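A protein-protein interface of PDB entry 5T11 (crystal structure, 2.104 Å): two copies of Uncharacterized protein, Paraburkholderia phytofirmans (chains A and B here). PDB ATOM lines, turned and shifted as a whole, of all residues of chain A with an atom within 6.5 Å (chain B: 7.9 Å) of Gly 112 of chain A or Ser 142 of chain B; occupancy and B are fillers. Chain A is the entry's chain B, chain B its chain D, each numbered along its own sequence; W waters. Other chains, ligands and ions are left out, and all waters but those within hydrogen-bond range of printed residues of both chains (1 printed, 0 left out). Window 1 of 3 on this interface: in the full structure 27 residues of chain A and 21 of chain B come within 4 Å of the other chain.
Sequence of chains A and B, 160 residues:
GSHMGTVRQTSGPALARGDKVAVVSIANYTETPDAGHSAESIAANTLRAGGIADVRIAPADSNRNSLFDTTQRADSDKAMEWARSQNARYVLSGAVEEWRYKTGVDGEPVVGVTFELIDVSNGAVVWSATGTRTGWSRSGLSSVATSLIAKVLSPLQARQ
The side-chain hydroxyl of Thr 132 of chain A lies within hydrogen-bond range of the side-chain hydroxyl of Ser 143 of chain B, 2.6 Å away.
N of Leu 141 of chain B lies within hydrogen-bond range of OE1 of Glu 98 of chain A, 3.5 Å away.
The side-chain carboxylate (OE2) of Glu 98 of chain A is in hydrogen-bond range of the side-chain hydroxyl (OH) of Tyr 101 of chain B (2.5 Å).
The side-chain carboxylate (OE1) of Glu 98 of chain A is in hydrogen-bond range of the backbone NH (N) of Ser 142 of chain B (2.8 Å).
The side-chain hydroxyl (OG1) of Thr 146 of chain B sits at hydrogen-bond distance from the backbone carbonyl oxygen (O) of Ser 142 of chain B (2.8 Å).
The backbone NH (N) of Glu 97 of chain A lies within hydrogen-bond range of the backbone carbonyl oxygen (O) of Gly 112 of chain A (2.8 Å).
OE1 of Glu 97 of chain A lies close to N of Val 113 of chain A, at 3.2 Å.
OG1 of Thr 114 of chain A lies within hydrogen-bond range of OE2 of Glu 97 of chain A (2.6 Å).
The backbone NH (N) of Gly 112 of chain A sits at hydrogen-bond distance from the backbone carbonyl oxygen (O) of Glu 98 of chain A.
OH of Tyr 101 of chain B is in hydrogen-bond range of N of Leu 141 of chain B (2.9 Å).
Among the printed residues, pairs that only touch across the chains: Glu 97 of chain A with Ser 38 of chain B, Glu 97 of chain A with Ile 42 of chain B, Val 110 of chain A with Tyr 101 of chain B, Val 111 of chain A with Ser 142 of chain B, Gly 112 of chain A with Ser 142 of chain B, Thr 130 of chain A with Thr 146 of chain B, Thr 132 of chain A with Ser 142 of chain B and Thr 132 of chain A with Thr 146 of chain B.
Gly 112 of chain A touches one residue of chain B.
Of the printed residues of chain A, Ile 42 of chain B touches Glu 97 (3.97 Å).
Of the printed residues of chain A, Tyr 101 of chain B touches Glu 98 (2.5 Å) and Val 110 (3.7 Å).
Ser 142 of chain B touches just these residues of chain A: Glu 98, Val 111, Gly 112 and Thr 132.
Printed residues of chain A within 4 Å of Ser 143 of chain B: Thr 132 (2.6 Å).
Printed residues of chain A within 4 Å of Thr 146 of chain B: Thr 130 and Thr 132.
The nearest residue of chain B that does not touch Gly 112 of chain A is Ser 143 of chain B (6.3 Å).
The nearest printed residue of chain A that does not touch Thr 146 of chain B is Thr 6 of chain A (4.2 Å).
Of the 17 printed residues of chain B, 7 touch a printed residue of chain A.
Hydrophobic or aromatic side chains of chain A within 4 Å of the printed part of chain B: Val 110.
Positions printed for both chains: 99, 111 and 148.
Of the 12 pairs that touch across the chains among the printed residues, none has its exchanged pair printed and touching as well.
Water W1 lies within hydrogen-bond range of OG1 of Thr 130 of chain A (2.4 Å) and O of Ile 42 of chain B (2.9 Å).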
ATOM      1  N   THR A   6      -0.690 -31.782  13.272  1.00  0.00           N
ATOM      2  CA  THR A   6      -1.630 -32.599  12.517  1.00  0.00           C
ATOM      3  C   THR A   6      -0.900 -33.331  11.403  1.00  0.00           C
ATOM      4  O   THR A   6       0.077 -32.827  10.843  1.00  0.00           O
ATOM      5  CB  THR A   6      -2.743 -31.767  11.874  1.00  0.00           C
ATOM      6  OG1 THR A   6      -2.148 -30.688  11.131  1.00  0.00           O
ATOM      7  CG2 THR A   6      -3.693 -31.215  12.929  1.00  0.00           C
ATOM      8  N   THR A  30      10.807 -21.712   3.597  1.00  0.00           N
ATOM      9  CA  THR A  30      11.179 -21.060   4.837  1.00  0.00           C
ATOM     10  C   THR A  30      12.404 -20.197   4.601  1.00  0.00           C
ATOM     11  O   THR A  30      13.037 -20.224   3.543  1.00  0.00           O
ATOM     12  CB  THR A  30      11.492 -22.089   5.924  1.00  0.00           C
ATOM     13  OG1 THR A  30      12.844 -22.555   5.744  1.00  0.00           O
ATOM     14  CG2 THR A  30      10.526 -23.283   5.818  1.00  0.00           C
ATOM     15  N   ALA A  95       7.410 -30.061  -0.223  1.00  0.00           N
ATOM     16  CA  ALA A  95       7.833 -28.718   0.152  1.00  0.00           C
ATOM     17  C   ALA A  95       7.873 -28.580   1.669  1.00  0.00           C
ATOM     18  O   ALA A  95       7.104 -29.226   2.396  1.00  0.00           O
ATOM     19  CB  ALA A  95       6.904 -27.650  -0.435  1.00  0.00           C
ATOM     20  N   VAL A  96       8.766 -27.710   2.131  1.00  0.00           N
ATOM     21  CA  VAL A  96       8.859 -27.345   3.538  1.00  0.00           C
ATOM     22  C   VAL A  96       8.201 -25.977   3.716  1.00  0.00           C
ATOM     23  O   VAL A  96       8.651 -24.977   3.140  1.00  0.00           O
ATOM     24  CB  VAL A  96      10.320 -27.347   4.014  1.00  0.00           C
ATOM     25  CG1 VAL A  96      10.410 -26.964   5.482  1.00  0.00           C
ATOM     26  CG2 VAL A  96      10.951 -28.749   3.766  1.00  0.00           C
ATOM     27  N   GLU A  97       7.107 -25.940   4.483  1.00  0.00           N
ATOM     28  CA  GLU A  97       6.387 -24.702   4.773  1.00  0.00           C
ATOM     29  C   GLU A  97       6.888 -24.007   6.027  1.00  0.00           C
ATOM     30  O   GLU A  97       6.681 -22.794   6.178  1.00  0.00           O
ATOM     31  CB  GLU A  97       4.877 -24.979   4.928  1.00  0.00           C
ATOM     32  CG  GLU A  97       4.174 -25.386   3.620  1.00  0.00           C
ATOM     33  CD  GLU A  97       4.351 -26.862   3.284  1.00  0.00           C
ATOM     34  OE1 GLU A  97       4.447 -27.680   4.232  1.00  0.00           O
ATOM     35  OE2 GLU A  97       4.411 -27.205   2.077  1.00  0.00           O
ATOM     36  N   GLU A  98       7.540 -24.737   6.928  1.00  0.00           N
ATOM     37  CA  GLU A  98       8.036 -24.144   8.162  1.00  0.00           C
ATOM     38  C   GLU A  98       9.099 -25.062   8.737  1.00  0.00           C
ATOM     39  O   GLU A  98       8.961 -26.291   8.700  1.00  0.00           O
ATOM     40  CB  GLU A  98       6.900 -23.930   9.172  1.00  0.00           C
ATOM     41  CG  GLU A  98       7.353 -23.370  10.503  1.00  0.00           C
ATOM     42  CD  GLU A  98       6.215 -22.687  11.283  1.00  0.00           C
ATOM     43  OE1 GLU A  98       5.109 -23.279  11.385  1.00  0.00           O
ATOM     44  OE2 GLU A  98       6.439 -21.554  11.801  1.00  0.00           O
ATOM     45  N   TRP A  99      10.150 -24.461   9.272  1.00  0.00           N
ATOM     46  CA  TRP A  99      11.310 -25.195   9.757  1.00  0.00           C
ATOM     47  C   TRP A  99      12.196 -24.226  10.526  1.00  0.00           C
ATOM     48  O   TRP A  99      13.203 -23.746   9.994  1.00  0.00           O
ATOM     49  CB  TRP A  99      12.058 -25.808   8.574  1.00  0.00           C
ATOM     50  CG  TRP A  99      13.151 -26.831   8.861  1.00  0.00           C
ATOM     51  CD1 TRP A  99      14.385 -26.595   9.410  1.00  0.00           C
ATOM     52  CD2 TRP A  99      13.131 -28.232   8.512  1.00  0.00           C
ATOM     53  NE1 TRP A  99      15.118 -27.764   9.453  1.00  0.00           N
ATOM     54  CE2 TRP A  99      14.370 -28.783   8.917  1.00  0.00           C
ATOM     55  CE3 TRP A  99      12.172 -29.075   7.929  1.00  0.00           C
ATOM     56  CZ2 TRP A  99      14.684 -30.143   8.741  1.00  0.00           C
ATOM     57  CZ3 TRP A  99      12.486 -30.423   7.754  1.00  0.00           C
ATOM     58  CH2 TRP A  99      13.739 -30.938   8.157  1.00  0.00           C
ATOM     59  N   VAL A 110       9.337 -25.628  15.305  1.00  0.00           N
ATOM     60  CA  VAL A 110       8.102 -25.829  14.556  1.00  0.00           C
ATOM     61  C   VAL A 110       8.458 -26.305  13.149  1.00  0.00           C
ATOM     62  O   VAL A 110       9.383 -25.779  12.520  1.00  0.00           O
ATOM     63  CB  VAL A 110       7.248 -24.538  14.512  1.00  0.00           C
ATOM     64  CG1 VAL A 110       6.702 -24.188  15.899  1.00  0.00           C
ATOM     65  CG2 VAL A 110       8.078 -23.383  14.015  1.00  0.00           C
ATOM     66  N   VAL A 111       7.716 -27.295  12.650  1.00  0.00           N
ATOM     67  CA  VAL A 111       7.976 -27.912  11.347  1.00  0.00           C
ATOM     68  C   VAL A 111       6.663 -28.099  10.597  1.00  0.00           C
ATOM     69  O   VAL A 111       5.683 -28.603  11.160  1.00  0.00           O
ATOM     70  CB  VAL A 111       8.683 -29.276  11.494  1.00  0.00           C
ATOM     71  CG1 VAL A 111       8.894 -29.937  10.122  1.00  0.00           C
ATOM     72  CG2 VAL A 111      10.025 -29.110  12.226  1.00  0.00           C
ATOM     73  N   GLY A 112       6.644 -27.703   9.323  1.00  0.00           N
ATOM     74  CA  GLY A 112       5.527 -27.986   8.433  1.00  0.00           C
ATOM     75  C   GLY A 112       6.046 -28.505   7.097  1.00  0.00           C
ATOM     76  O   GLY A 112       6.968 -27.901   6.534  1.00  0.00           O
ATOM     77  N   VAL A 113       5.501 -29.633   6.599  1.00  0.00           N
ATOM     78  CA  VAL A 113       5.973 -30.294   5.381  1.00  0.00           C
ATOM     79  C   VAL A 113       4.784 -30.853   4.606  1.00  0.00           C
ATOM     80  O   VAL A 113       3.795 -31.308   5.189  1.00  0.00           O
ATOM     81  CB  VAL A 113       6.967 -31.443   5.667  1.00  0.00           C
ATOM     82  CG1 VAL A 113       8.247 -30.920   6.269  1.00  0.00           C
ATOM     83  CG2 VAL A 113       6.329 -32.495   6.579  1.00  0.00           C
ATOM     84  N   THR A 114       4.896 -30.829   3.277  1.00  0.00           N
ATOM     85  CA  THR A 114       3.964 -31.509   2.386  1.00  0.00           C
ATOM     86  C   THR A 114       4.763 -32.444   1.481  1.00  0.00           C
ATOM     87  O   THR A 114       5.880 -32.114   1.069  1.00  0.00           O
ATOM     88  CB  THR A 114       3.153 -30.502   1.549  1.00  0.00           C
ATOM     89  OG1 THR A 114       4.046 -29.529   0.989  1.00  0.00           O
ATOM     90  CG2 THR A 114       2.104 -29.773   2.408  1.00  0.00           C
ATOM     91  N   THR A 130       0.379 -34.156   4.342  1.00  0.00           N
ATOM     92  CA  THR A 130       0.786 -32.925   5.001  1.00  0.00           C
ATOM     93  C   THR A 130       0.945 -33.211   6.486  1.00  0.00           C
ATOM     94  O   THR A 130       0.111 -33.907   7.090  1.00  0.00           O
ATOM     95  CB  THR A 130      -0.250 -31.804   4.798  1.00  0.00           C
ATOM     96  OG1 THR A 130      -0.494 -31.618   3.393  1.00  0.00           O
ATOM     97  CG2 THR A 130       0.241 -30.481   5.416  1.00  0.00           C
ATOM     98  N   GLY A 131       2.027 -32.687   7.071  1.00  0.00           N
ATOM     99  CA  GLY A 131       2.261 -32.879   8.490  1.00  0.00           C
ATOM    100  C   GLY A 131       2.811 -31.615   9.120  1.00  0.00           C
ATOM    101  O   GLY A 131       3.600 -30.905   8.483  1.00  0.00           O
ATOM    102  N   THR A 132       2.393 -31.300  10.347  1.00  0.00           N
ATOM    103  CA  THR A 132       2.942 -30.174  11.089  1.00  0.00           C
ATOM    104  C   THR A 132       3.188 -30.624  12.519  1.00  0.00           C
ATOM    105  O   THR A 132       2.520 -31.538  13.010  1.00  0.00           O
ATOM    106  CB  THR A 132       2.008 -28.938  11.092  1.00  0.00           C
ATOM    107  OG1 THR A 132       0.817 -29.224  11.848  1.00  0.00           O
ATOM    108  CG2 THR A 132       1.618 -28.530   9.669  1.00  0.00           C
ATOM    109  N   ARG A 133       4.133 -29.964  13.193  1.00  0.00           N
ATOM    110  CA  ARG A 133       4.383 -30.285  14.593  1.00  0.00           C
ATOM    111  C   ARG A 133       5.046 -29.111  15.306  1.00  0.00           C
ATOM    112  O   ARG A 133       5.832 -28.363  14.713  1.00  0.00           O
ATOM    113  CB  ARG A 133       5.249 -31.546  14.734  1.00  0.00           C
ATOM    114  CG  ARG A 133       5.430 -31.996  16.178  1.00  0.00           C
ATOM    115  CD  ARG A 133       6.096 -33.346  16.260  1.00  0.00           C
ATOM    116  NE  ARG A 133       5.255 -34.389  15.687  1.00  0.00           N
ATOM    117  CZ  ARG A 133       5.578 -35.677  15.667  1.00  0.00           C
ATOM    118  NH1 ARG A 133       6.728 -36.070  16.192  1.00  0.00           N
ATOM    119  NH2 ARG A 133       4.754 -36.567  15.127  1.00  0.00           N
ATOM    120  N   LEU A 148       8.592 -36.176  12.813  1.00  0.00           N
ATOM    121  CA  LEU A 148       7.378 -35.858  12.062  1.00  0.00           C
ATOM    122  C   LEU A 148       7.394 -36.485  10.671  1.00  0.00           C
ATOM    123  O   LEU A 148       6.381 -37.033  10.209  1.00  0.00           O
ATOM    124  CB  LEU A 148       7.208 -34.342  11.945  1.00  0.00           C
ATOM    125  CG  LEU A 148       6.085 -33.878  11.007  1.00  0.00           C
ATOM    126  CD1 LEU A 148       4.711 -34.283  11.561  1.00  0.00           C
ATOM    127  CD2 LEU A 148       6.128 -32.348  10.744  1.00  0.00           C
ATOM    128  N   SER B  38       3.468 -21.711  -0.070  1.00  0.00           N
ATOM    129  CA  SER B  38       3.073 -22.607   1.010  1.00  0.00           C
ATOM    130  C   SER B  38       1.585 -22.870   0.969  1.00  0.00           C
ATOM    131  O   SER B  38       1.149 -24.024   1.053  1.00  0.00           O
ATOM    132  CB  SER B  38       3.474 -22.019   2.367  1.00  0.00           C
ATOM    133  OG  SER B  38       4.883 -22.045   2.455  1.00  0.00           O
ATOM    134  N   ILE B  42      -0.217 -26.591   0.445  1.00  0.00           N
ATOM    135  CA  ILE B  42      -1.162 -27.098   1.430  1.00  0.00           C
ATOM    136  C   ILE B  42      -2.548 -27.245   0.811  1.00  0.00           C
ATOM    137  O   ILE B  42      -3.246 -28.242   1.047  1.00  0.00           O
ATOM    138  CB  ILE B  42      -1.188 -26.170   2.663  1.00  0.00           C
ATOM    139  CG1 ILE B  42       0.158 -26.209   3.402  1.00  0.00           C
ATOM    140  CG2 ILE B  42      -2.344 -26.549   3.601  1.00  0.00           C
ATOM    141  CD1 ILE B  42       0.306 -25.113   4.471  1.00  0.00           C
ATOM    142  N   TRP B  99      -0.125 -14.144   7.314  1.00  0.00           N
ATOM    143  CA  TRP B  99       0.617 -15.387   7.486  1.00  0.00           C
ATOM    144  C   TRP B  99       1.910 -15.100   8.246  1.00  0.00           C
ATOM    145  O   TRP B  99       2.988 -15.008   7.646  1.00  0.00           O
ATOM    146  CB  TRP B  99       0.894 -16.006   6.114  1.00  0.00           C
ATOM    147  CG  TRP B  99       1.418 -17.424   6.067  1.00  0.00           C
ATOM    148  CD1 TRP B  99       2.652 -17.874   6.486  1.00  0.00           C
ATOM    149  CD2 TRP B  99       0.759 -18.560   5.476  1.00  0.00           C
ATOM    150  NE1 TRP B  99       2.779 -19.223   6.219  1.00  0.00           N
ATOM    151  CE2 TRP B  99       1.637 -19.665   5.597  1.00  0.00           C
ATOM    152  CE3 TRP B  99      -0.496 -18.751   4.873  1.00  0.00           C
ATOM    153  CZ2 TRP B  99       1.301 -20.940   5.140  1.00  0.00           C
ATOM    154  CZ3 TRP B  99      -0.828 -20.023   4.413  1.00  0.00           C
ATOM    155  CH2 TRP B  99       0.071 -21.098   4.550  1.00  0.00           C
ATOM    156  N   TYR B 101       3.749 -14.770  12.619  1.00  0.00           N
ATOM    157  CA  TYR B 101       3.591 -14.705  14.062  1.00  0.00           C
ATOM    158  C   TYR B 101       3.473 -13.238  14.428  1.00  0.00           C
ATOM    159  O   TYR B 101       4.236 -12.417  13.915  1.00  0.00           O
ATOM    160  CB  TYR B 101       4.784 -15.321  14.801  1.00  0.00           C
ATOM    161  CG  TYR B 101       4.953 -16.798  14.564  1.00  0.00           C
ATOM    162  CD1 TYR B 101       4.216 -17.714  15.303  1.00  0.00           C
ATOM    163  CD2 TYR B 101       5.842 -17.277  13.603  1.00  0.00           C
ATOM    164  CE1 TYR B 101       4.346 -19.066  15.106  1.00  0.00           C
ATOM    165  CE2 TYR B 101       5.982 -18.670  13.379  1.00  0.00           C
ATOM    166  CZ  TYR B 101       5.225 -19.548  14.150  1.00  0.00           C
ATOM    167  OH  TYR B 101       5.305 -20.913  13.992  1.00  0.00           O
ATOM    168  N   PRO B 109       0.546 -17.148  16.169  1.00  0.00           N
ATOM    169  CA  PRO B 109       0.393 -17.166  14.711  1.00  0.00           C
ATOM    170  C   PRO B 109      -0.984 -16.685  14.278  1.00  0.00           C
ATOM    171  O   PRO B 109      -1.994 -16.917  14.947  1.00  0.00           O
ATOM    172  CB  PRO B 109       0.593 -18.641  14.358  1.00  0.00           C
ATOM    173  CG  PRO B 109       0.114 -19.382  15.571  1.00  0.00           C
ATOM    174  CD  PRO B 109       0.484 -18.504  16.752  1.00  0.00           C
ATOM    175  N   VAL B 111      -3.373 -16.338  10.509  1.00  0.00           N
ATOM    176  CA  VAL B 111      -3.490 -16.646   9.087  1.00  0.00           C
ATOM    177  C   VAL B 111      -4.789 -16.064   8.545  1.00  0.00           C
ATOM    178  O   VAL B 111      -5.842 -16.180   9.180  1.00  0.00           O
ATOM    179  CB  VAL B 111      -3.444 -18.168   8.841  1.00  0.00           C
ATOM    180  CG1 VAL B 111      -3.593 -18.491   7.344  1.00  0.00           C
ATOM    181  CG2 VAL B 111      -2.154 -18.745   9.416  1.00  0.00           C
ATOM    182  N   SER B 139       1.354 -22.164  19.612  1.00  0.00           N
ATOM    183  CA  SER B 139       0.990 -22.971  18.460  1.00  0.00           C
ATOM    184  C   SER B 139       1.865 -22.622  17.259  1.00  0.00           C
ATOM    185  O   SER B 139       2.519 -21.576  17.210  1.00  0.00           O
ATOM    186  CB  SER B 139      -0.496 -22.810  18.120  1.00  0.00           C
ATOM    187  OG  SER B 139      -0.797 -21.514  17.656  1.00  0.00           O
ATOM    188  N   GLY B 140       1.890 -23.542  16.298  1.00  0.00           N
ATOM    189  CA  GLY B 140       2.713 -23.386  15.117  1.00  0.00           C
ATOM    190  C   GLY B 140       1.941 -22.703  14.003  1.00  0.00           C
ATOM    191  O   GLY B 140       0.764 -22.983  13.784  1.00  0.00           O
ATOM    192  N   LEU B 141       2.625 -21.783  13.312  1.00  0.00           N
ATOM    193  CA  LEU B 141       2.024 -21.107  12.167  1.00  0.00           C
ATOM    194  C   LEU B 141       1.569 -22.115  11.114  1.00  0.00           C
ATOM    195  O   LEU B 141       0.449 -22.029  10.594  1.00  0.00           O
ATOM    196  CB  LEU B 141       3.019 -20.112  11.569  1.00  0.00           C
ATOM    197  CG  LEU B 141       2.623 -19.295  10.333  1.00  0.00           C
ATOM    198  CD1 LEU B 141       1.295 -18.587  10.550  1.00  0.00           C
ATOM    199  CD2 LEU B 141       3.732 -18.247  10.020  1.00  0.00           C
ATOM    200  N   SER B 142       2.421 -23.090  10.792  1.00  0.00           N
ATOM    201  CA  SER B 142       2.024 -24.041   9.770  1.00  0.00           C
ATOM    202  C   SER B 142       0.873 -24.929  10.238  1.00  0.00           C
ATOM    203  O   SER B 142       0.065 -25.365   9.409  1.00  0.00           O
ATOM    204  CB  SER B 142       3.219 -24.890   9.317  1.00  0.00           C
ATOM    205  OG  SER B 142       3.865 -25.555  10.392  1.00  0.00           O
ATOM    206  N   SER B 143       0.785 -25.219  11.542  1.00  0.00           N
ATOM    207  CA  SER B 143      -0.357 -25.985  12.045  1.00  0.00           C
ATOM    208  C   SER B 143      -1.647 -25.203  11.884  1.00  0.00           C
ATOM    209  O   SER B 143      -2.674 -25.763  11.483  1.00  0.00           O
ATOM    210  CB  SER B 143      -0.162 -26.360  13.516  1.00  0.00           C
ATOM    211  OG  SER B 143       0.876 -27.315  13.683  1.00  0.00           O
ATOM    212  N   VAL B 144      -1.613 -23.905  12.192  1.00  0.00           N
ATOM    213  CA  VAL B 144      -2.822 -23.097  12.092  1.00  0.00           C
ATOM    214  C   VAL B 144      -3.239 -22.933  10.630  1.00  0.00           C
ATOM    215  O   VAL B 144      -4.425 -23.040  10.290  1.00  0.00           O
ATOM    216  CB  VAL B 144      -2.611 -21.745  12.803  1.00  0.00           C
ATOM    217  CG1 VAL B 144      -3.729 -20.774  12.450  1.00  0.00           C
ATOM    218  CG2 VAL B 144      -2.562 -21.957  14.327  1.00  0.00           C
ATOM    219  N   ALA B 145      -2.272 -22.710   9.741  1.00  0.00           N
ATOM    220  CA  ALA B 145      -2.586 -22.563   8.322  1.00  0.00           C
ATOM    221  C   ALA B 145      -3.157 -23.845   7.739  1.00  0.00           C
ATOM    222  O   ALA B 145      -4.120 -23.804   6.966  1.00  0.00           O
ATOM    223  CB  ALA B 145      -1.340 -22.161   7.537  1.00  0.00           C
ATOM    224  N   THR B 146      -2.538 -24.986   8.049  1.00  0.00           N
ATOM    225  CA  THR B 146      -3.017 -26.260   7.522  1.00  0.00           C
ATOM    226  C   THR B 146      -4.430 -26.551   8.014  1.00  0.00           C
ATOM    227  O   THR B 146      -5.324 -26.886   7.225  1.00  0.00           O
ATOM    228  CB  THR B 146      -2.050 -27.374   7.925  1.00  0.00           C
ATOM    229  OG1 THR B 146      -0.764 -27.125   7.333  1.00  0.00           O
ATOM    230  CG2 THR B 146      -2.534 -28.691   7.424  1.00  0.00           C
ATOM    231  N   SER B 147      -4.655 -26.405   9.321  1.00  0.00           N
ATOM    232  CA  SER B 147      -5.986 -26.642   9.861  1.00  0.00           C
ATOM    233  C   SER B 147      -7.006 -25.694   9.240  1.00  0.00           C
ATOM    234  O   SER B 147      -8.119 -26.113   8.889  1.00  0.00           O
ATOM    235  CB  SER B 147      -5.960 -26.499  11.384  1.00  0.00           C
ATOM    236  OG  SER B 147      -7.243 -26.708  11.935  1.00  0.00           O
ATOM    237  N   LEU B 148      -6.642 -24.414   9.071  1.00  0.00           N
ATOM    238  CA  LEU B 148      -7.596 -23.452   8.515  1.00  0.00           C
ATOM    239  C   LEU B 148      -7.919 -23.777   7.062  1.00  0.00           C
ATOM    240  O   LEU B 148      -9.084 -23.753   6.652  1.00  0.00           O
ATOM    241  CB  LEU B 148      -7.056 -22.026   8.630  1.00  0.00           C
ATOM    242  CG  LEU B 148      -7.813 -20.875   7.938  1.00  0.00           C
ATOM    243  CD1 LEU B 148      -9.255 -20.707   8.446  1.00  0.00           C
ATOM    244  CD2 LEU B 148      -7.047 -19.525   8.116  1.00  0.00           C
ATOM    245  N   ILE B 149      -6.898 -24.081   6.267  1.00  0.00           N
ATOM    246  CA  ILE B 149      -7.125 -24.279   4.841  1.00  0.00           C
ATOM    247  C   ILE B 149      -7.988 -25.513   4.606  1.00  0.00           C
ATOM    248  O   ILE B 149      -8.873 -25.511   3.740  1.00  0.00           O
ATOM    249  CB  ILE B 149      -5.772 -24.342   4.107  1.00  0.00           C
ATOM    250  CG1 ILE B 149      -5.190 -22.918   4.046  1.00  0.00           C
ATOM    251  CG2 ILE B 149      -5.933 -24.966   2.714  1.00  0.00           C
ATOM    252  CD1 ILE B 149      -3.740 -22.806   3.621  1.00  0.00           C
HETATM  253  O   HOH W   1      -2.304 -30.046   3.145  1.00  0.00           O
